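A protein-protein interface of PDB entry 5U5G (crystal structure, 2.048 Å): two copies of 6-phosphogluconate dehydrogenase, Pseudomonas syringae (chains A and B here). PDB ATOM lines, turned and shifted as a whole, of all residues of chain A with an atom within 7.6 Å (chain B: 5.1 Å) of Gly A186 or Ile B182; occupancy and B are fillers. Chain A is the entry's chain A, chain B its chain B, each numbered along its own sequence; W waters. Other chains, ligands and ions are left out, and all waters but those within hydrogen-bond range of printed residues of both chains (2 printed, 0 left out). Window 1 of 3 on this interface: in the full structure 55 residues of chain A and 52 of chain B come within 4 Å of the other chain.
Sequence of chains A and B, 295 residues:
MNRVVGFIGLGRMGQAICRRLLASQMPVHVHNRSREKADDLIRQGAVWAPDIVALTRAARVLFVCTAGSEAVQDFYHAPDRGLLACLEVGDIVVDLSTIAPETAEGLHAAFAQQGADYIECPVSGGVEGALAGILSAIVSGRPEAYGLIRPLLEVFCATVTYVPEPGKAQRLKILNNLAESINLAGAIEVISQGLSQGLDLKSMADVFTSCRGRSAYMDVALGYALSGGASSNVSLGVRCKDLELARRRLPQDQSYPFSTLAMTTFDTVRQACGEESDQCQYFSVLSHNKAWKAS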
ATOM      1  N   ALA A 179     -23.383  17.951  14.416  1.00  0.00           N
ATOM      2  CA  ALA A 179     -22.967  19.025  13.507  1.00  0.00           C
ATOM      3  C   ALA A 179     -22.075  18.494  12.389  1.00  0.00           C
ATOM      4  O   ALA A 179     -22.168  18.951  11.242  1.00  0.00           O
ATOM      5  CB  ALA A 179     -22.249  20.130  14.286  1.00  0.00           C
ATOM      6  N   GLU A 180     -21.197  17.534  12.711  1.00  0.00           N
ATOM      7  CA  GLU A 180     -20.440  16.828  11.678  1.00  0.00           C
ATOM      8  C   GLU A 180     -21.372  16.269  10.620  1.00  0.00           C
ATOM      9  O   GLU A 180     -21.151  16.442   9.415  1.00  0.00           O
ATOM     10  CB  GLU A 180     -19.650  15.670  12.297  1.00  0.00           C
ATOM     11  CG  GLU A 180     -18.612  16.072  13.316  1.00  0.00           C
ATOM     12  CD  GLU A 180     -17.806  14.884  13.820  1.00  0.00           C
ATOM     13  OE1 GLU A 180     -18.271  13.742  13.641  1.00  0.00           O
ATOM     14  OE2 GLU A 180     -16.714  15.104  14.401  1.00  0.00           O
ATOM     15  N   SER A 181     -22.410  15.566  11.074  1.00  0.00           N
ATOM     16  CA  SER A 181     -23.308  14.856  10.175  1.00  0.00           C
ATOM     17  C   SER A 181     -24.027  15.827   9.252  1.00  0.00           C
ATOM     18  O   SER A 181     -24.175  15.564   8.051  1.00  0.00           O
ATOM     19  CB  SER A 181     -24.309  14.034  10.988  1.00  0.00           C
ATOM     20  OG  SER A 181     -23.641  13.255  11.975  1.00  0.00           O
ATOM     21  N   ILE A 182     -24.473  16.959   9.796  1.00  0.00           N
ATOM     22  CA  ILE A 182     -25.131  17.972   8.975  1.00  0.00           C
ATOM     23  C   ILE A 182     -24.146  18.574   7.979  1.00  0.00           C
ATOM     24  O   ILE A 182     -24.467  18.755   6.799  1.00  0.00           O
ATOM     25  CB  ILE A 182     -25.753  19.061   9.864  1.00  0.00           C
ATOM     26  CG1 ILE A 182     -26.871  18.458  10.725  1.00  0.00           C
ATOM     27  CG2 ILE A 182     -26.282  20.182   8.978  1.00  0.00           C
ATOM     28  CD1 ILE A 182     -27.245  19.307  11.975  1.00  0.00           C
ATOM     29  N   ASN A 183     -22.938  18.920   8.452  1.00  0.00           N
ATOM     30  CA  ASN A 183     -21.930  19.499   7.569  1.00  0.00           C
ATOM     31  C   ASN A 183     -21.556  18.534   6.456  1.00  0.00           C
ATOM     32  O   ASN A 183     -21.376  18.943   5.298  1.00  0.00           O
ATOM     33  CB  ASN A 183     -20.665  19.871   8.355  1.00  0.00           C
ATOM     34  CG  ASN A 183     -20.910  20.971   9.383  1.00  0.00           C
ATOM     35  OD1 ASN A 183     -21.967  21.589   9.400  1.00  0.00           O
ATOM     36  ND2 ASN A 183     -19.922  21.221  10.229  1.00  0.00           N
ATOM     37  N   LEU A 184     -21.374  17.256   6.807  1.00  0.00           N
ATOM     38  CA  LEU A 184     -20.969  16.253   5.832  1.00  0.00           C
ATOM     39  C   LEU A 184     -22.037  16.063   4.771  1.00  0.00           C
ATOM     40  O   LEU A 184     -21.736  16.044   3.574  1.00  0.00           O
ATOM     41  CB  LEU A 184     -20.668  14.928   6.536  1.00  0.00           C
ATOM     42  CG  LEU A 184     -20.247  13.758   5.622  1.00  0.00           C
ATOM     43  CD1 LEU A 184     -19.031  14.123   4.775  1.00  0.00           C
ATOM     44  CD2 LEU A 184     -19.952  12.512   6.445  1.00  0.00           C
ATOM     45  N   ALA A 185     -23.299  15.910   5.189  1.00  0.00           N
ATOM     46  CA  ALA A 185     -24.364  15.716   4.210  1.00  0.00           C
ATOM     47  C   ALA A 185     -24.529  16.944   3.325  1.00  0.00           C
ATOM     48  O   ALA A 185     -24.765  16.819   2.119  1.00  0.00           O
ATOM     49  CB  ALA A 185     -25.678  15.382   4.910  1.00  0.00           C
ATOM     50  N   GLY A 186     -24.410  18.140   3.903  1.00  0.00           N
ATOM     51  CA  GLY A 186     -24.464  19.344   3.086  1.00  0.00           C
ATOM     52  C   GLY A 186     -23.303  19.425   2.113  1.00  0.00           C
ATOM     53  O   GLY A 186     -23.481  19.761   0.937  1.00  0.00           O
ATOM     54  N   ALA A 187     -22.090  19.114   2.593  1.00  0.00           N
ATOM     55  CA  ALA A 187     -20.919  19.224   1.729  1.00  0.00           C
ATOM     56  C   ALA A 187     -21.015  18.254   0.561  1.00  0.00           C
ATOM     57  O   ALA A 187     -20.696  18.613  -0.578  1.00  0.00           O
ATOM     58  CB  ALA A 187     -19.634  18.995   2.535  1.00  0.00           C
ATOM     59  N   ILE A 188     -21.505  17.033   0.810  1.00  0.00           N
ATOM     60  CA  ILE A 188     -21.687  16.060  -0.272  1.00  0.00           C
ATOM     61  C   ILE A 188     -22.746  16.537  -1.265  1.00  0.00           C
ATOM     62  O   ILE A 188     -22.613  16.344  -2.483  1.00  0.00           O
ATOM     63  CB  ILE A 188     -22.020  14.669   0.309  1.00  0.00           C
ATOM     64  CG1 ILE A 188     -20.814  14.117   1.065  1.00  0.00           C
ATOM     65  CG2 ILE A 188     -22.411  13.687  -0.803  1.00  0.00           C
ATOM     66  CD1 ILE A 188     -21.062  12.765   1.721  1.00  0.00           C
ATOM     67  N   GLU A 189     -23.804  17.181  -0.777  1.00  0.00           N
ATOM     68  CA  GLU A 189     -24.796  17.716  -1.704  1.00  0.00           C
ATOM     69  C   GLU A 189     -24.211  18.839  -2.549  1.00  0.00           C
ATOM     70  O   GLU A 189     -24.470  18.920  -3.753  1.00  0.00           O
ATOM     71  CB  GLU A 189     -26.025  18.203  -0.940  1.00  0.00           C
ATOM     72  CG  GLU A 189     -26.892  17.065  -0.446  1.00  0.00           C
ATOM     73  CD  GLU A 189     -28.191  17.551   0.158  1.00  0.00           C
ATOM     74  OE1 GLU A 189     -28.613  18.681  -0.175  1.00  0.00           O
ATOM     75  OE2 GLU A 189     -28.795  16.807   0.951  1.00  0.00           O
ATOM     76  N   VAL A 190     -23.402  19.702  -1.940  1.00  0.00           N
ATOM     77  CA  VAL A 190     -22.863  20.840  -2.670  1.00  0.00           C
ATOM     78  C   VAL A 190     -21.821  20.386  -3.689  1.00  0.00           C
ATOM     79  O   VAL A 190     -21.823  20.837  -4.841  1.00  0.00           O
ATOM     80  CB  VAL A 190     -22.315  21.864  -1.661  1.00  0.00           C
ATOM     81  CG1 VAL A 190     -21.308  22.786  -2.297  1.00  0.00           C
ATOM     82  CG2 VAL A 190     -23.493  22.658  -1.079  1.00  0.00           C
ATOM     83  N   ILE A 191     -20.938  19.465  -3.296  1.00  0.00           N
ATOM     84  CA  ILE A 191     -19.968  18.911  -4.238  1.00  0.00           C
ATOM     85  C   ILE A 191     -20.684  18.218  -5.388  1.00  0.00           C
ATOM     86  O   ILE A 191     -20.312  18.381  -6.557  1.00  0.00           O
ATOM     87  CB  ILE A 191     -19.001  17.949  -3.519  1.00  0.00           C
ATOM     88  CG1 ILE A 191     -18.149  18.712  -2.502  1.00  0.00           C
ATOM     89  CG2 ILE A 191     -18.125  17.231  -4.540  1.00  0.00           C
ATOM     90  CD1 ILE A 191     -17.430  17.820  -1.526  1.00  0.00           C
ATOM     91  N   SER A 192     -21.735  17.452  -5.077  1.00  0.00           N
ATOM     92  CA  SER A 192     -22.438  16.702  -6.116  1.00  0.00           C
ATOM     93  C   SER A 192     -23.083  17.638  -7.128  1.00  0.00           C
ATOM     94  O   SER A 192     -22.982  17.423  -8.344  1.00  0.00           O
ATOM     95  CB  SER A 192     -23.492  15.789  -5.492  1.00  0.00           C
ATOM     96  OG  SER A 192     -22.865  14.839  -4.655  1.00  0.00           O
ATOM     97  N   GLN A 193     -23.773  18.668  -6.637  1.00  0.00           N
ATOM     98  CA  GLN A 193     -24.369  19.659  -7.526  1.00  0.00           C
ATOM     99  C   GLN A 193     -23.309  20.315  -8.396  1.00  0.00           C
ATOM    100  O   GLN A 193     -23.513  20.495  -9.603  1.00  0.00           O
ATOM    101  CB  GLN A 193     -25.123  20.711  -6.705  1.00  0.00           C
ATOM    102  CG  GLN A 193     -26.355  20.141  -6.044  1.00  0.00           C
ATOM    103  CD  GLN A 193     -27.069  21.138  -5.156  1.00  0.00           C
ATOM    104  OE1 GLN A 193     -27.630  22.132  -5.640  1.00  0.00           O
ATOM    105  NE2 GLN A 193     -27.069  20.874  -3.846  1.00  0.00           N
ATOM    106  N   MET A 218     -16.357  19.241   5.428  1.00  0.00           N
ATOM    107  CA  MET A 218     -16.156  19.547   4.014  1.00  0.00           C
ATOM    108  C   MET A 218     -14.804  19.021   3.535  1.00  0.00           C
ATOM    109  O   MET A 218     -14.705  18.439   2.446  1.00  0.00           O
ATOM    110  CB  MET A 218     -16.261  21.058   3.776  1.00  0.00           C
ATOM    111  CG  MET A 218     -15.821  21.516   2.370  1.00  0.00           C
ATOM    112  SD  MET A 218     -16.801  20.939   0.955  1.00  0.00           S
ATOM    113  CE  MET A 218     -18.240  22.022   1.081  1.00  0.00           C
ATOM    114  N   ALA A 221     -15.225  15.365   2.993  1.00  0.00           N
ATOM    115  CA  ALA A 221     -15.977  15.056   1.785  1.00  0.00           C
ATOM    116  C   ALA A 221     -15.143  15.314   0.534  1.00  0.00           C
ATOM    117  O   ALA A 221     -15.192  14.534  -0.425  1.00  0.00           O
ATOM    118  CB  ALA A 221     -17.264  15.877   1.756  1.00  0.00           C
ATOM    119  N   PHE A 258     -32.925  20.150  10.698  1.00  0.00           N
ATOM    120  CA  PHE A 258     -31.639  19.714  10.155  1.00  0.00           C
ATOM    121  C   PHE A 258     -31.101  18.513  10.918  1.00  0.00           C
ATOM    122  O   PHE A 258     -30.579  17.572  10.307  1.00  0.00           O
ATOM    123  CB  PHE A 258     -30.630  20.864  10.151  1.00  0.00           C
ATOM    124  CG  PHE A 258     -30.772  21.780   8.955  1.00  0.00           C
ATOM    125  CD1 PHE A 258     -31.577  22.904   9.017  1.00  0.00           C
ATOM    126  CD2 PHE A 258     -30.132  21.485   7.761  1.00  0.00           C
ATOM    127  CE1 PHE A 258     -31.722  23.735   7.907  1.00  0.00           C
ATOM    128  CE2 PHE A 258     -30.268  22.305   6.654  1.00  0.00           C
ATOM    129  CZ  PHE A 258     -31.063  23.445   6.731  1.00  0.00           C
ATOM    130  N   PHE A 266     -28.645   9.470   7.193  1.00  0.00           N
ATOM    131  CA  PHE A 266     -27.561   8.505   7.324  1.00  0.00           C
ATOM    132  C   PHE A 266     -28.092   7.117   7.667  1.00  0.00           C
ATOM    133  O   PHE A 266     -27.451   6.111   7.332  1.00  0.00           O
ATOM    134  CB  PHE A 266     -26.527   9.003   8.333  1.00  0.00           C
ATOM    135  CG  PHE A 266     -25.622  10.078   7.772  1.00  0.00           C
ATOM    136  CD1 PHE A 266     -24.539   9.737   6.953  1.00  0.00           C
ATOM    137  CD2 PHE A 266     -25.876  11.430   8.020  1.00  0.00           C
ATOM    138  CE1 PHE A 266     -23.707  10.723   6.409  1.00  0.00           C
ATOM    139  CE2 PHE A 266     -25.043  12.424   7.496  1.00  0.00           C
ATOM    140  CZ  PHE A 266     -23.962  12.077   6.678  1.00  0.00           C
ATOM    141  N   TYR A 282     -23.027   8.524   1.169  1.00  0.00           N
ATOM    142  CA  TYR A 282     -24.102   9.415   0.744  1.00  0.00           C
ATOM    143  C   TYR A 282     -23.890   9.896  -0.693  1.00  0.00           C
ATOM    144  O   TYR A 282     -24.864  10.120  -1.414  1.00  0.00           O
ATOM    145  CB  TYR A 282     -24.199  10.612   1.695  1.00  0.00           C
ATOM    146  CG  TYR A 282     -25.405  11.525   1.462  1.00  0.00           C
ATOM    147  CD1 TYR A 282     -26.645  11.004   1.117  1.00  0.00           C
ATOM    148  CD2 TYR A 282     -25.302  12.903   1.642  1.00  0.00           C
ATOM    149  CE1 TYR A 282     -27.756  11.839   0.935  1.00  0.00           C
ATOM    150  CE2 TYR A 282     -26.403  13.745   1.460  1.00  0.00           C
ATOM    151  CZ  TYR A 282     -27.621  13.209   1.118  1.00  0.00           C
ATOM    152  OH  TYR A 282     -28.698  14.055   0.939  1.00  0.00           O
ATOM    153  N   LEU A 286     -26.917   9.583  -3.143  1.00  0.00           N
ATOM    154  CA  LEU A 286     -27.446  10.810  -3.725  1.00  0.00           C
ATOM    155  C   LEU A 286     -27.744  10.630  -5.209  1.00  0.00           C
ATOM    156  O   LEU A 286     -28.847  10.939  -5.672  1.00  0.00           O
ATOM    157  CB  LEU A 286     -26.451  11.947  -3.497  1.00  0.00           C
ATOM    158  CG  LEU A 286     -26.961  13.369  -3.348  1.00  0.00           C
ATOM    159  CD1 LEU A 286     -28.308  13.423  -2.656  1.00  0.00           C
ATOM    160  CD2 LEU A 286     -25.918  14.123  -2.557  1.00  0.00           C
ATOM    161  N   LEU B 178     -24.295  27.927  -0.172  1.00  0.00           N
ATOM    162  CA  LEU B 178     -25.225  26.867   0.206  1.00  0.00           C
ATOM    163  C   LEU B 178     -24.669  26.057   1.365  1.00  0.00           C
ATOM    164  O   LEU B 178     -25.380  25.773   2.334  1.00  0.00           O
ATOM    165  CB  LEU B 178     -25.486  25.955  -0.991  1.00  0.00           C
ATOM    166  CG  LEU B 178     -26.903  25.506  -1.320  1.00  0.00           C
ATOM    167  CD1 LEU B 178     -26.844  24.235  -2.159  1.00  0.00           C
ATOM    168  CD2 LEU B 178     -27.782  25.335  -0.090  1.00  0.00           C
ATOM    169  N   ALA B 179     -23.391  25.660   1.271  1.00  0.00           N
ATOM    170  CA  ALA B 179     -22.726  25.013   2.402  1.00  0.00           C
ATOM    171  C   ALA B 179     -22.740  25.900   3.645  1.00  0.00           C
ATOM    172  O   ALA B 179     -22.976  25.412   4.757  1.00  0.00           O
ATOM    173  CB  ALA B 179     -21.285  24.639   2.040  1.00  0.00           C
ATOM    174  N   GLU B 180     -22.464  27.200   3.484  1.00  0.00           N
ATOM    175  CA  GLU B 180     -22.553  28.114   4.625  1.00  0.00           C
ATOM    176  C   GLU B 180     -23.925  28.029   5.293  1.00  0.00           C
ATOM    177  O   GLU B 180     -24.032  27.939   6.525  1.00  0.00           O
ATOM    178  CB  GLU B 180     -22.292  29.557   4.184  1.00  0.00           C
ATOM    179  CG  GLU B 180     -20.861  29.874   3.752  1.00  0.00           C
ATOM    180  CD  GLU B 180     -20.715  31.325   3.335  1.00  0.00           C
ATOM    181  OE1 GLU B 180     -21.723  32.050   3.364  1.00  0.00           O
ATOM    182  OE2 GLU B 180     -19.595  31.751   2.979  1.00  0.00           O
ATOM    183  N   SER B 181     -24.991  28.059   4.479  1.00  0.00           N
ATOM    184  CA  SER B 181     -26.343  28.102   5.029  1.00  0.00           C
ATOM    185  C   SER B 181     -26.669  26.820   5.778  1.00  0.00           C
ATOM    186  O   SER B 181     -27.228  26.866   6.880  1.00  0.00           O
ATOM    187  CB  SER B 181     -27.354  28.343   3.915  1.00  0.00           C
ATOM    188  OG  SER B 181     -27.060  29.548   3.230  1.00  0.00           O
ATOM    189  N   ILE B 182     -26.321  25.669   5.197  1.00  0.00           N
ATOM    190  CA  ILE B 182     -26.539  24.395   5.875  1.00  0.00           C
ATOM    191  C   ILE B 182     -25.743  24.338   7.177  1.00  0.00           C
ATOM    192  O   ILE B 182     -26.275  23.975   8.239  1.00  0.00           O
ATOM    193  CB  ILE B 182     -26.192  23.225   4.931  1.00  0.00           C
ATOM    194  CG1 ILE B 182     -27.165  23.202   3.736  1.00  0.00           C
ATOM    195  CG2 ILE B 182     -26.203  21.924   5.698  1.00  0.00           C
ATOM    196  CD1 ILE B 182     -26.705  22.339   2.515  1.00  0.00           C
ATOM    197  N   ASN B 183     -24.455  24.700   7.115  1.00  0.00           N
ATOM    198  CA  ASN B 183     -23.618  24.688   8.308  1.00  0.00           C
ATOM    199  C   ASN B 183     -24.176  25.607   9.384  1.00  0.00           C
ATOM    200  O   ASN B 183     -24.180  25.256  10.576  1.00  0.00           O
ATOM    201  CB  ASN B 183     -22.185  25.107   7.963  1.00  0.00           C
ATOM    202  CG  ASN B 183     -21.483  24.094   7.069  1.00  0.00           C
ATOM    203  OD1 ASN B 183     -22.059  23.060   6.719  1.00  0.00           O
ATOM    204  ND2 ASN B 183     -20.242  24.388   6.695  1.00  0.00           N
ATOM    205  N   LEU B 184     -24.637  26.794   8.978  1.00  0.00           N
ATOM    206  CA  LEU B 184     -25.149  27.773   9.926  1.00  0.00           C
ATOM    207  C   LEU B 184     -26.397  27.251  10.616  1.00  0.00           C
ATOM    208  O   LEU B 184     -26.513  27.305  11.847  1.00  0.00           O
ATOM    209  CB  LEU B 184     -25.450  29.092   9.210  1.00  0.00           C
ATOM    210  CG  LEU B 184     -26.061  30.200  10.095  1.00  0.00           C
ATOM    211  CD1 LEU B 184     -25.161  30.523  11.281  1.00  0.00           C
ATOM    212  CD2 LEU B 184     -26.334  31.464   9.274  1.00  0.00           C
ATOM    213  N   ALA B 185     -27.361  26.775   9.827  1.00  0.00           N
ATOM    214  CA  ALA B 185     -28.580  26.215  10.398  1.00  0.00           C
ATOM    215  C   ALA B 185     -28.258  25.085  11.362  1.00  0.00           C
ATOM    216  O   ALA B 185     -28.791  25.032  12.476  1.00  0.00           O
ATOM    217  CB  ALA B 185     -29.488  25.720   9.286  1.00  0.00           C
ATOM    218  N   GLY B 186     -27.369  24.180  10.953  1.00  0.00           N
ATOM    219  CA  GLY B 186     -26.991  23.084  11.827  1.00  0.00           C
ATOM    220  C   GLY B 186     -26.329  23.554  13.107  1.00  0.00           C
ATOM    221  O   GLY B 186     -26.640  23.059  14.195  1.00  0.00           O
ATOM    222  N   ALA B 187     -25.392  24.500  12.992  1.00  0.00           N
ATOM    223  CA  ALA B 187     -24.725  25.053  14.170  1.00  0.00           C
ATOM    224  C   ALA B 187     -25.739  25.629  15.151  1.00  0.00           C
ATOM    225  O   ALA B 187     -25.681  25.372  16.357  1.00  0.00           O
ATOM    226  CB  ALA B 187     -23.712  26.128  13.751  1.00  0.00           C
ATOM    227  N   PHE B 258     -30.935  18.486   2.114  1.00  0.00           N
ATOM    228  CA  PHE B 258     -30.330  19.516   2.961  1.00  0.00           C
ATOM    229  C   PHE B 258     -30.304  20.877   2.272  1.00  0.00           C
ATOM    230  O   PHE B 258     -30.521  21.911   2.921  1.00  0.00           O
ATOM    231  CB  PHE B 258     -28.921  19.097   3.381  1.00  0.00           C
ATOM    232  CG  PHE B 258     -28.907  18.154   4.550  1.00  0.00           C
ATOM    233  CD1 PHE B 258     -29.017  16.790   4.353  1.00  0.00           C
ATOM    234  CD2 PHE B 258     -28.800  18.639   5.854  1.00  0.00           C
ATOM    235  CE1 PHE B 258     -29.031  15.913   5.440  1.00  0.00           C
ATOM    236  CE2 PHE B 258     -28.807  17.774   6.936  1.00  0.00           C
ATOM    237  CZ  PHE B 258     -28.926  16.404   6.725  1.00  0.00           C
ATOM    238  N   SER B 259     -30.026  20.898   0.963  1.00  0.00           N
ATOM    239  CA  SER B 259     -30.010  22.145   0.201  1.00  0.00           C
ATOM    240  C   SER B 259     -31.390  22.786   0.174  1.00  0.00           C
ATOM    241  O   SER B 259     -31.536  23.995   0.391  1.00  0.00           O
ATOM    242  CB  SER B 259     -29.533  21.876  -1.230  1.00  0.00           C
ATOM    243  OG  SER B 259     -28.282  21.223  -1.231  1.00  0.00           O
ATOM    244  N   ALA B 262     -32.362  24.131   3.602  1.00  0.00           N
ATOM    245  CA  ALA B 262     -31.732  25.420   3.855  1.00  0.00           C
ATOM    246  C   ALA B 262     -32.484  26.551   3.169  1.00  0.00           C
ATOM    247  O   ALA B 262     -32.678  27.612   3.763  1.00  0.00           O
ATOM    248  CB  ALA B 262     -30.276  25.394   3.396  1.00  0.00           C
HETATM  249  O   HOH W   1     -21.660  21.631   4.457  1.00  0.00           O
HETATM  250  O   HOH W   2     -22.875  22.931  11.656  1.00  0.00           O
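OD1 of Asn A183 sits close to OD1 of Asn B183, 3.1 Å away. The backbone NH (N) of Phe B258 is in hydrogen-bond range of the side-chain carboxylate (OE2) of Glu A189 (3.0 Å). OE1 of Glu A189 lies within hydrogen-bond range of OG of Ser B259 (2.8 Å). OG of Ser B259 lies within hydrogen-bond range of NE2 of Gln A193.
The backbone carbonyl oxygen of Ala A179 lies close to the side-chain amide oxygen of Asn A183 (3.2 Å). O of Glu A189 lies close to NE2 of Gln A193. The side-chain carboxylate (OE2) of Glu A189 is in hydrogen-bond range of the side-chain hydroxyl (OH) of Tyr A282 (2.8 Å). OD1 of Asn B183 sits close to O of Ala B179.
Among the printed residues, pairs that only touch across the chains: Phe A258 with Ala B185 (3.3 Å), Ala A185 with Phe B258 (3.4 Å), Phe A258 with Ala B262 (3.5 Å), Phe A258 with Phe B258 (3.7 Å), Ile A182 with Ile B182 (3.7 Å), Gln A193 with Leu B178 (3.8 Å), Gly A186 with Ile B182 (3.8 Å), Ile A182 with Gly B186 (3.8 Å), Val A190 with Ala B179 (3.8 Å) and Val A190 with Leu B178 (3.9 Å).
Gly A186 touches one residue of chain B. Of the printed residues of chain A, Ala B179 touches Val A190. Printed residues of chain A within 4 Å of Phe B258: Ala A185 (3.4 Å), Glu A189 (3.0 Å) and Phe A258 (3.7 Å). Of the printed residues of chain B, Val A190 touches Leu B178 (3.9 Å) and Ala B179 (3.8 Å). Of the printed residues of chain B, Ile A182 touches Ile B182 and Gly B186. Of the printed residues of chain A, Ala B262 touches Phe A258 (3.5 Å). Leu B184 touches none of the printed residues of chain A. Ile A191 touches none of the printed residues of chain B. The nearest residue of chain A that does not touch Ile B182 is Phe A258 (4.2 Å).
Of the 13 printed residues of chain B, 9 touch a printed residue of chain A. Along chain B the printed residues that touch a printed residue of chain A span positions 178 to 262. Of the 21 printed residues of chain A, 8 touch a printed residue of chain B. Among the printed residues, 14 pairs touch across the chains. Among the printed residues, no Asp or Glu carboxylate lies within 4 Å of a Lys or Arg side-chain nitrogen of the other chain.
Ile A182 touches its own counterpart, Ile B182. Ile A182 touches Gly B186, and with the chains exchanged Gly A186 touches Ile B182. Asn A183 touches its own counterpart, Asn B183. Phe A258 touches its own counterpart, Phe B258.
Water W1 lies within hydrogen-bond range of OD1 of Asn B183 (2.7 Å), O of Asn A183 (2.8 Å) and N of Ala A187 (3.2 Å). Water W2 lies within hydrogen-bond range of the side-chain amide oxygen of Asn A183, the backbone carbonyl oxygen of Asn B183 and the backbone NH of Ala B187.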
